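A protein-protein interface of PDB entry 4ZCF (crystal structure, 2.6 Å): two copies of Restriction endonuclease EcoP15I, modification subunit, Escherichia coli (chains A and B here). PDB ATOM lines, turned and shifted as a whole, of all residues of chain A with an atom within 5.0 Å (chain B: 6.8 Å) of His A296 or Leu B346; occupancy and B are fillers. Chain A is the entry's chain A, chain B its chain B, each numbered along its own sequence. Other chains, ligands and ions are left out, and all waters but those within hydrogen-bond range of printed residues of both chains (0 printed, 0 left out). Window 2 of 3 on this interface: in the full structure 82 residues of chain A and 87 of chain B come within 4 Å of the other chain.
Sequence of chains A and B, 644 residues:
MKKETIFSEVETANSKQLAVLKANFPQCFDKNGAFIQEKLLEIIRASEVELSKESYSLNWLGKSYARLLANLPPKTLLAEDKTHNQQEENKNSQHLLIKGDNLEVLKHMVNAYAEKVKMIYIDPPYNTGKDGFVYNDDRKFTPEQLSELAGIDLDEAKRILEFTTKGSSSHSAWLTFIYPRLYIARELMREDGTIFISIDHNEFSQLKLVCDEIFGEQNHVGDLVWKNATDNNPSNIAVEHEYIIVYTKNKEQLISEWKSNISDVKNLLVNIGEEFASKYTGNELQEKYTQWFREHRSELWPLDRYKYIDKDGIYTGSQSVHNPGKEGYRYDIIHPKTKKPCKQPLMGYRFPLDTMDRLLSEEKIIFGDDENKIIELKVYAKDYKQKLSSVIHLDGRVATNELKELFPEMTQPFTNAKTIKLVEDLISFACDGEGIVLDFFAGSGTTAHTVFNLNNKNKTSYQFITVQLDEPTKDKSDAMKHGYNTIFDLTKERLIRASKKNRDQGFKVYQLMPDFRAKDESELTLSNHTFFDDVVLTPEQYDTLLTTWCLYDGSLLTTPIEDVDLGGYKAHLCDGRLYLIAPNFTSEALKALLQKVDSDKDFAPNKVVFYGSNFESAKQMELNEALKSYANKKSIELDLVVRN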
ATOM      1  N   LEU A 268      -4.382   2.616   5.903  1.00  0.00           N
ATOM      2  CA  LEU A 268      -4.103   3.992   5.483  1.00  0.00           C
ATOM      3  C   LEU A 268      -5.299   4.893   5.771  1.00  0.00           C
ATOM      4  O   LEU A 268      -5.119   5.974   6.324  1.00  0.00           O
ATOM      5  CB  LEU A 268      -3.751   4.003   3.978  1.00  0.00           C
ATOM      6  CG  LEU A 268      -3.634   5.349   3.263  1.00  0.00           C
ATOM      7  CD1 LEU A 268      -2.242   5.932   3.406  1.00  0.00           C
ATOM      8  CD2 LEU A 268      -3.981   5.207   1.787  1.00  0.00           C
ATOM      9  N   TRP A 292      -9.151  16.062   0.249  1.00  0.00           N
ATOM     10  CA  TRP A 292      -8.117  15.027   0.207  1.00  0.00           C
ATOM     11  C   TRP A 292      -8.625  13.805  -0.559  1.00  0.00           C
ATOM     12  O   TRP A 292      -7.825  13.160  -1.241  1.00  0.00           O
ATOM     13  CB  TRP A 292      -7.689  14.643   1.629  1.00  0.00           C
ATOM     14  CG  TRP A 292      -6.648  13.555   1.714  1.00  0.00           C
ATOM     15  CD1 TRP A 292      -5.298  13.713   1.856  1.00  0.00           C
ATOM     16  CD2 TRP A 292      -6.894  12.142   1.746  1.00  0.00           C
ATOM     17  NE1 TRP A 292      -4.688  12.487   1.973  1.00  0.00           N
ATOM     18  CE2 TRP A 292      -5.645  11.504   1.899  1.00  0.00           C
ATOM     19  CE3 TRP A 292      -8.051  11.350   1.621  1.00  0.00           C
ATOM     20  CZ2 TRP A 292      -5.519  10.110   1.902  1.00  0.00           C
ATOM     21  CZ3 TRP A 292      -7.924   9.974   1.623  1.00  0.00           C
ATOM     22  CH2 TRP A 292      -6.675   9.366   1.776  1.00  0.00           C
ATOM     23  N   PHE A 293      -9.945  13.472  -0.416  1.00  0.00           N
ATOM     24  CA  PHE A 293     -10.569  12.371  -1.128  1.00  0.00           C
ATOM     25  C   PHE A 293     -10.603  12.647  -2.638  1.00  0.00           C
ATOM     26  O   PHE A 293     -10.120  11.799  -3.402  1.00  0.00           O
ATOM     27  CB  PHE A 293     -11.962  12.037  -0.577  1.00  0.00           C
ATOM     28  CG  PHE A 293     -12.581  10.818  -1.213  1.00  0.00           C
ATOM     29  CD1 PHE A 293     -12.199   9.536  -0.822  1.00  0.00           C
ATOM     30  CD2 PHE A 293     -13.546  10.945  -2.205  1.00  0.00           C
ATOM     31  CE1 PHE A 293     -12.793   8.404  -1.396  1.00  0.00           C
ATOM     32  CE2 PHE A 293     -14.142   9.816  -2.774  1.00  0.00           C
ATOM     33  CZ  PHE A 293     -13.762   8.556  -2.364  1.00  0.00           C
ATOM     34  N   ARG A 294     -11.118  13.843  -3.068  1.00  0.00           N
ATOM     35  CA  ARG A 294     -11.175  14.230  -4.492  1.00  0.00           C
ATOM     36  C   ARG A 294      -9.834  14.056  -5.219  1.00  0.00           C
ATOM     37  O   ARG A 294      -9.821  13.542  -6.333  1.00  0.00           O
ATOM     38  CB  ARG A 294     -11.695  15.650  -4.660  1.00  0.00           C
ATOM     39  N   GLU A 295      -8.718  14.390  -4.550  1.00  0.00           N
ATOM     40  CA  GLU A 295      -7.363  14.247  -5.096  1.00  0.00           C
ATOM     41  C   GLU A 295      -6.761  12.815  -5.056  1.00  0.00           C
ATOM     42  O   GLU A 295      -6.056  12.431  -5.994  1.00  0.00           O
ATOM     43  CB  GLU A 295      -6.408  15.243  -4.421  1.00  0.00           C
ATOM     44  CG  GLU A 295      -5.391  15.834  -5.386  1.00  0.00           C
ATOM     45  CD  GLU A 295      -3.938  15.840  -4.944  1.00  0.00           C
ATOM     46  OE1 GLU A 295      -3.660  15.596  -3.745  1.00  0.00           O
ATOM     47  OE2 GLU A 295      -3.070  16.110  -5.806  1.00  0.00           O
ATOM     48  N   HIS A 296      -7.027  12.043  -3.976  1.00  0.00           N
ATOM     49  CA  HIS A 296      -6.448  10.712  -3.763  1.00  0.00           C
ATOM     50  C   HIS A 296      -7.280   9.497  -4.190  1.00  0.00           C
ATOM     51  O   HIS A 296      -6.708   8.426  -4.364  1.00  0.00           O
ATOM     52  CB  HIS A 296      -5.931  10.569  -2.324  1.00  0.00           C
ATOM     53  CG  HIS A 296      -4.842  11.541  -1.974  1.00  0.00           C
ATOM     54  ND1 HIS A 296      -5.122  12.868  -1.700  1.00  0.00           N
ATOM     55  CD2 HIS A 296      -3.509  11.342  -1.857  1.00  0.00           C
ATOM     56  CE1 HIS A 296      -3.957  13.428  -1.426  1.00  0.00           C
ATOM     57  NE2 HIS A 296      -2.956  12.548  -1.510  1.00  0.00           N
ATOM     58  N   ARG A 297      -8.605   9.670  -4.379  1.00  0.00           N
ATOM     59  CA  ARG A 297      -9.609   8.670  -4.790  1.00  0.00           C
ATOM     60  C   ARG A 297      -9.060   7.567  -5.746  1.00  0.00           C
ATOM     61  O   ARG A 297      -9.291   6.373  -5.521  1.00  0.00           O
ATOM     62  CB  ARG A 297     -10.819   9.410  -5.416  1.00  0.00           C
ATOM     63  CG  ARG A 297     -12.023   8.543  -5.766  1.00  0.00           C
ATOM     64  CD  ARG A 297     -13.262   9.345  -6.154  1.00  0.00           C
ATOM     65  NE  ARG A 297     -13.120  10.066  -7.424  1.00  0.00           N
ATOM     66  CZ  ARG A 297     -13.116  11.393  -7.547  1.00  0.00           C
ATOM     67  NH1 ARG A 297     -13.249  12.168  -6.476  1.00  0.00           N
ATOM     68  NH2 ARG A 297     -12.986  11.956  -8.742  1.00  0.00           N
ATOM     69  N   SER A 298      -8.316   7.994  -6.780  1.00  0.00           N
ATOM     70  CA  SER A 298      -7.702   7.177  -7.838  1.00  0.00           C
ATOM     71  C   SER A 298      -6.689   6.135  -7.346  1.00  0.00           C
ATOM     72  O   SER A 298      -6.375   5.210  -8.096  1.00  0.00           O
ATOM     73  CB  SER A 298      -7.039   8.082  -8.876  1.00  0.00           C
ATOM     74  OG  SER A 298      -6.033   8.889  -8.280  1.00  0.00           O
ATOM     75  N   GLU A 299      -6.174   6.288  -6.110  1.00  0.00           N
ATOM     76  CA  GLU A 299      -5.174   5.416  -5.472  1.00  0.00           C
ATOM     77  C   GLU A 299      -5.809   4.492  -4.404  1.00  0.00           C
ATOM     78  O   GLU A 299      -5.119   3.639  -3.839  1.00  0.00           O
ATOM     79  CB  GLU A 299      -4.126   6.299  -4.751  1.00  0.00           C
ATOM     80  CG  GLU A 299      -3.417   7.342  -5.610  1.00  0.00           C
ATOM     81  CD  GLU A 299      -2.412   8.172  -4.837  1.00  0.00           C
ATOM     82  OE1 GLU A 299      -2.619   9.401  -4.707  1.00  0.00           O
ATOM     83  OE2 GLU A 299      -1.435   7.583  -4.323  1.00  0.00           O
ATOM     84  N   LEU A 300      -7.109   4.683  -4.118  1.00  0.00           N
ATOM     85  CA  LEU A 300      -7.846   4.017  -3.057  1.00  0.00           C
ATOM     86  C   LEU A 300      -8.466   2.669  -3.324  1.00  0.00           C
ATOM     87  O   LEU A 300      -9.013   2.096  -2.378  1.00  0.00           O
ATOM     88  CB  LEU A 300      -8.850   4.983  -2.388  1.00  0.00           C
ATOM     89  CG  LEU A 300      -8.237   6.293  -1.823  1.00  0.00           C
ATOM     90  CD1 LEU A 300      -9.295   7.201  -1.227  1.00  0.00           C
ATOM     91  CD2 LEU A 300      -7.101   6.024  -0.841  1.00  0.00           C
ATOM     92  N   HIS B 322       1.297   3.470  -9.167  1.00  0.00           N
ATOM     93  CA  HIS B 322       1.100   3.058  -7.786  1.00  0.00           C
ATOM     94  C   HIS B 322       0.745   1.606  -7.717  1.00  0.00           C
ATOM     95  O   HIS B 322       0.321   1.029  -8.715  1.00  0.00           O
ATOM     96  CB  HIS B 322       0.003   3.907  -7.118  1.00  0.00           C
ATOM     97  CG  HIS B 322      -1.398   3.497  -7.466  1.00  0.00           C
ATOM     98  ND1 HIS B 322      -1.980   3.865  -8.669  1.00  0.00           N
ATOM     99  CD2 HIS B 322      -2.292   2.780  -6.746  1.00  0.00           C
ATOM    100  CE1 HIS B 322      -3.200   3.348  -8.650  1.00  0.00           C
ATOM    101  NE2 HIS B 322      -3.434   2.688  -7.512  1.00  0.00           N
ATOM    102  N   ASN B 323       0.875   1.020  -6.529  1.00  0.00           N
ATOM    103  CA  ASN B 323       0.520  -0.375  -6.345  1.00  0.00           C
ATOM    104  C   ASN B 323      -0.960  -0.477  -5.868  1.00  0.00           C
ATOM    105  O   ASN B 323      -1.322   0.147  -4.856  1.00  0.00           O
ATOM    106  CB  ASN B 323       1.515  -1.063  -5.409  1.00  0.00           C
ATOM    107  CG  ASN B 323       1.764  -2.517  -5.735  1.00  0.00           C
ATOM    108  OD1 ASN B 323       1.386  -3.037  -6.798  1.00  0.00           O
ATOM    109  ND2 ASN B 323       2.423  -3.209  -4.819  1.00  0.00           N
ATOM    110  N   GLU B 327       0.791  -2.240  -0.470  1.00  0.00           N
ATOM    111  CA  GLU B 327       1.983  -1.420  -0.281  1.00  0.00           C
ATOM    112  C   GLU B 327       3.037  -1.942  -1.258  1.00  0.00           C
ATOM    113  O   GLU B 327       3.235  -3.160  -1.375  1.00  0.00           O
ATOM    114  CB  GLU B 327       2.494  -1.520   1.171  1.00  0.00           C
ATOM    115  CG  GLU B 327       3.751  -0.711   1.460  1.00  0.00           C
ATOM    116  CD  GLU B 327       3.568   0.734   1.885  1.00  0.00           C
ATOM    117  OE1 GLU B 327       2.408   1.203   1.957  1.00  0.00           O
ATOM    118  OE2 GLU B 327       4.594   1.394   2.168  1.00  0.00           O
ATOM    119  N   ARG B 330       9.022   1.779  -2.170  1.00  0.00           N
ATOM    120  CA  ARG B 330       9.270   3.149  -1.719  1.00  0.00           C
ATOM    121  C   ARG B 330      10.688   3.575  -2.112  1.00  0.00           C
ATOM    122  O   ARG B 330      11.665   2.901  -1.786  1.00  0.00           O
ATOM    123  CB  ARG B 330       9.097   3.268  -0.195  1.00  0.00           C
ATOM    124  CG  ARG B 330       7.720   2.884   0.317  1.00  0.00           C
ATOM    125  CD  ARG B 330       6.737   4.024   0.222  1.00  0.00           C
ATOM    126  NE  ARG B 330       5.454   3.645   0.806  1.00  0.00           N
ATOM    127  CZ  ARG B 330       4.348   4.375   0.733  1.00  0.00           C
ATOM    128  NH1 ARG B 330       4.351   5.541   0.090  1.00  0.00           N
ATOM    129  NH2 ARG B 330       3.230   3.947   1.300  1.00  0.00           N
ATOM    130  N   LYS B 343       6.022  13.847  -5.374  1.00  0.00           N
ATOM    131  CA  LYS B 343       4.980  13.367  -4.474  1.00  0.00           C
ATOM    132  C   LYS B 343       4.826  11.866  -4.704  1.00  0.00           C
ATOM    133  O   LYS B 343       4.589  11.423  -5.833  1.00  0.00           O
ATOM    134  CB  LYS B 343       3.663  14.097  -4.759  1.00  0.00           C
ATOM    135  CG  LYS B 343       2.535  13.739  -3.803  1.00  0.00           C
ATOM    136  CD  LYS B 343       1.252  14.428  -4.221  1.00  0.00           C
ATOM    137  CE  LYS B 343       0.067  13.918  -3.456  1.00  0.00           C
ATOM    138  NZ  LYS B 343      -1.188  14.210  -4.184  1.00  0.00           N
ATOM    139  N   GLN B 344       5.034  11.089  -3.636  1.00  0.00           N
ATOM    140  CA  GLN B 344       4.990   9.636  -3.634  1.00  0.00           C
ATOM    141  C   GLN B 344       3.545   9.110  -3.601  1.00  0.00           C
ATOM    142  O   GLN B 344       2.693   9.716  -2.932  1.00  0.00           O
ATOM    143  CB  GLN B 344       5.776   9.122  -2.423  1.00  0.00           C
ATOM    144  CG  GLN B 344       6.752   7.990  -2.740  1.00  0.00           C
ATOM    145  CD  GLN B 344       7.304   7.314  -1.505  1.00  0.00           C
ATOM    146  OE1 GLN B 344       6.752   7.392  -0.399  1.00  0.00           O
ATOM    147  NE2 GLN B 344       8.402   6.603  -1.677  1.00  0.00           N
ATOM    148  N   PRO B 345       3.223   7.992  -4.290  1.00  0.00           N
ATOM    149  CA  PRO B 345       1.852   7.458  -4.199  1.00  0.00           C
ATOM    150  C   PRO B 345       1.606   6.895  -2.798  1.00  0.00           C
ATOM    151  O   PRO B 345       2.546   6.359  -2.191  1.00  0.00           O
ATOM    152  CB  PRO B 345       1.817   6.350  -5.259  1.00  0.00           C
ATOM    153  CG  PRO B 345       3.087   6.429  -5.996  1.00  0.00           C
ATOM    154  CD  PRO B 345       4.075   7.118  -5.113  1.00  0.00           C
ATOM    155  N   LEU B 346       0.375   7.026  -2.260  1.00  0.00           N
ATOM    156  CA  LEU B 346       0.068   6.537  -0.898  1.00  0.00           C
ATOM    157  C   LEU B 346       0.484   5.070  -0.624  1.00  0.00           C
ATOM    158  O   LEU B 346       0.837   4.749   0.509  1.00  0.00           O
ATOM    159  CB  LEU B 346      -1.401   6.736  -0.525  1.00  0.00           C
ATOM    160  CG  LEU B 346      -2.000   8.120  -0.682  1.00  0.00           C
ATOM    161  CD1 LEU B 346      -3.502   8.011  -0.865  1.00  0.00           C
ATOM    162  CD2 LEU B 346      -1.643   9.020   0.504  1.00  0.00           C
ATOM    163  N   MET B 347       0.451   4.197  -1.666  1.00  0.00           N
ATOM    164  CA  MET B 347       0.812   2.776  -1.555  1.00  0.00           C
ATOM    165  C   MET B 347       2.183   2.437  -2.143  1.00  0.00           C
ATOM    166  O   MET B 347       2.472   1.266  -2.360  1.00  0.00           O
ATOM    167  CB  MET B 347      -0.286   1.895  -2.186  1.00  0.00           C
ATOM    168  CG  MET B 347      -1.658   2.047  -1.543  1.00  0.00           C
ATOM    169  SD  MET B 347      -1.746   1.111  -0.012  1.00  0.00           S
ATOM    170  CE  MET B 347      -1.442   2.400   1.206  1.00  0.00           C
ATOM    171  N   GLY B 348       3.015   3.456  -2.385  1.00  0.00           N
ATOM    172  CA  GLY B 348       4.330   3.299  -2.996  1.00  0.00           C
ATOM    173  C   GLY B 348       4.204   2.968  -4.472  1.00  0.00           C
ATOM    174  O   GLY B 348       3.120   3.072  -5.050  1.00  0.00           O
ATOM    175  N   ILE B 374       2.161  13.459  -8.818  1.00  0.00           N
ATOM    176  CA  ILE B 374       2.674  12.085  -8.942  1.00  0.00           C
ATOM    177  C   ILE B 374       2.937  11.786 -10.423  1.00  0.00           C
ATOM    178  O   ILE B 374       2.182  12.243 -11.275  1.00  0.00           O
ATOM    179  CB  ILE B 374       1.704  11.033  -8.276  1.00  0.00           C
ATOM    180  CG1 ILE B 374       1.322  11.452  -6.825  1.00  0.00           C
ATOM    181  CG2 ILE B 374       2.293   9.596  -8.302  1.00  0.00           C
ATOM    182  CD1 ILE B 374       0.221  10.659  -6.184  1.00  0.00           C
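The side-chain carboxylate of Glu A295 lies within salt-bridge range of the side-chain amino group of Lys B343 (2.9 Å). The side-chain carboxylate (OE2) of Glu A299 sits at hydrogen-bond distance from the backbone NH (N) of Leu B346 (2.8 Å).
The backbone carbonyl oxygen (O) of Trp A292 is in hydrogen-bond range of a ring nitrogen (ND1) of His A296. The guanidinium group (NH1) of Arg B330 sits at hydrogen-bond distance from the backbone carbonyl oxygen (O) of Pro B345. The guanidinium group (NH2) of Arg B330 lies within hydrogen-bond range of the backbone carbonyl oxygen (O) of Leu B346, at 2.6 Å.
Leu A268 touches Leu B346. Leu A268 touches Met B347. His A296 touches Lys B343 (NE2 to NZ, 3.6 Å). His A296 touches Leu B346. Ser A298 touches His B322 (O to CE1, 3.7 Å). Glu A299 touches His B322. CA of Pro B345 touches OE2 of Glu A299, at 3.3 Å. Glu A299 touches Ile B374.
Arg A294 touches none of the printed residues of chain B. His A296 touches just these residues of chain B: Lys B343 (3.6 Å) and Leu B346 (3.5 Å). Of the printed residues of chain B, Glu A299 touches His B322, Pro B345, Leu B346 and Ile B374. Printed residues of chain A within 4 Å of Leu B346: Leu A268, His A296 and Glu A299. Of the printed residues of chain A, Ile B374 touches Glu A299. The nearest printed residue of chain A that does not touch Leu B346 is Trp A292 (4.02 Å). The nearest printed residue of chain A that does not touch His B322 is Leu A300 (5.4 Å).
Hydrophobic or aromatic side chains of chain A that line the printed part of chain B: Leu A268 and His A296. Of the 11 printed residues of chain B, 6 touch a printed residue of chain A. Hydrophobic or aromatic side chains of chain B within 4 Å of the printed part of chain A: His B322, Pro B345, Leu B346, Met B347 and Ile B374. Among the printed residues, Asp or Glu carboxylates within 4 Å of a Lys or Arg side-chain nitrogen of the other chain: Glu A295 with Lys B343.
No position is printed for both chains.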
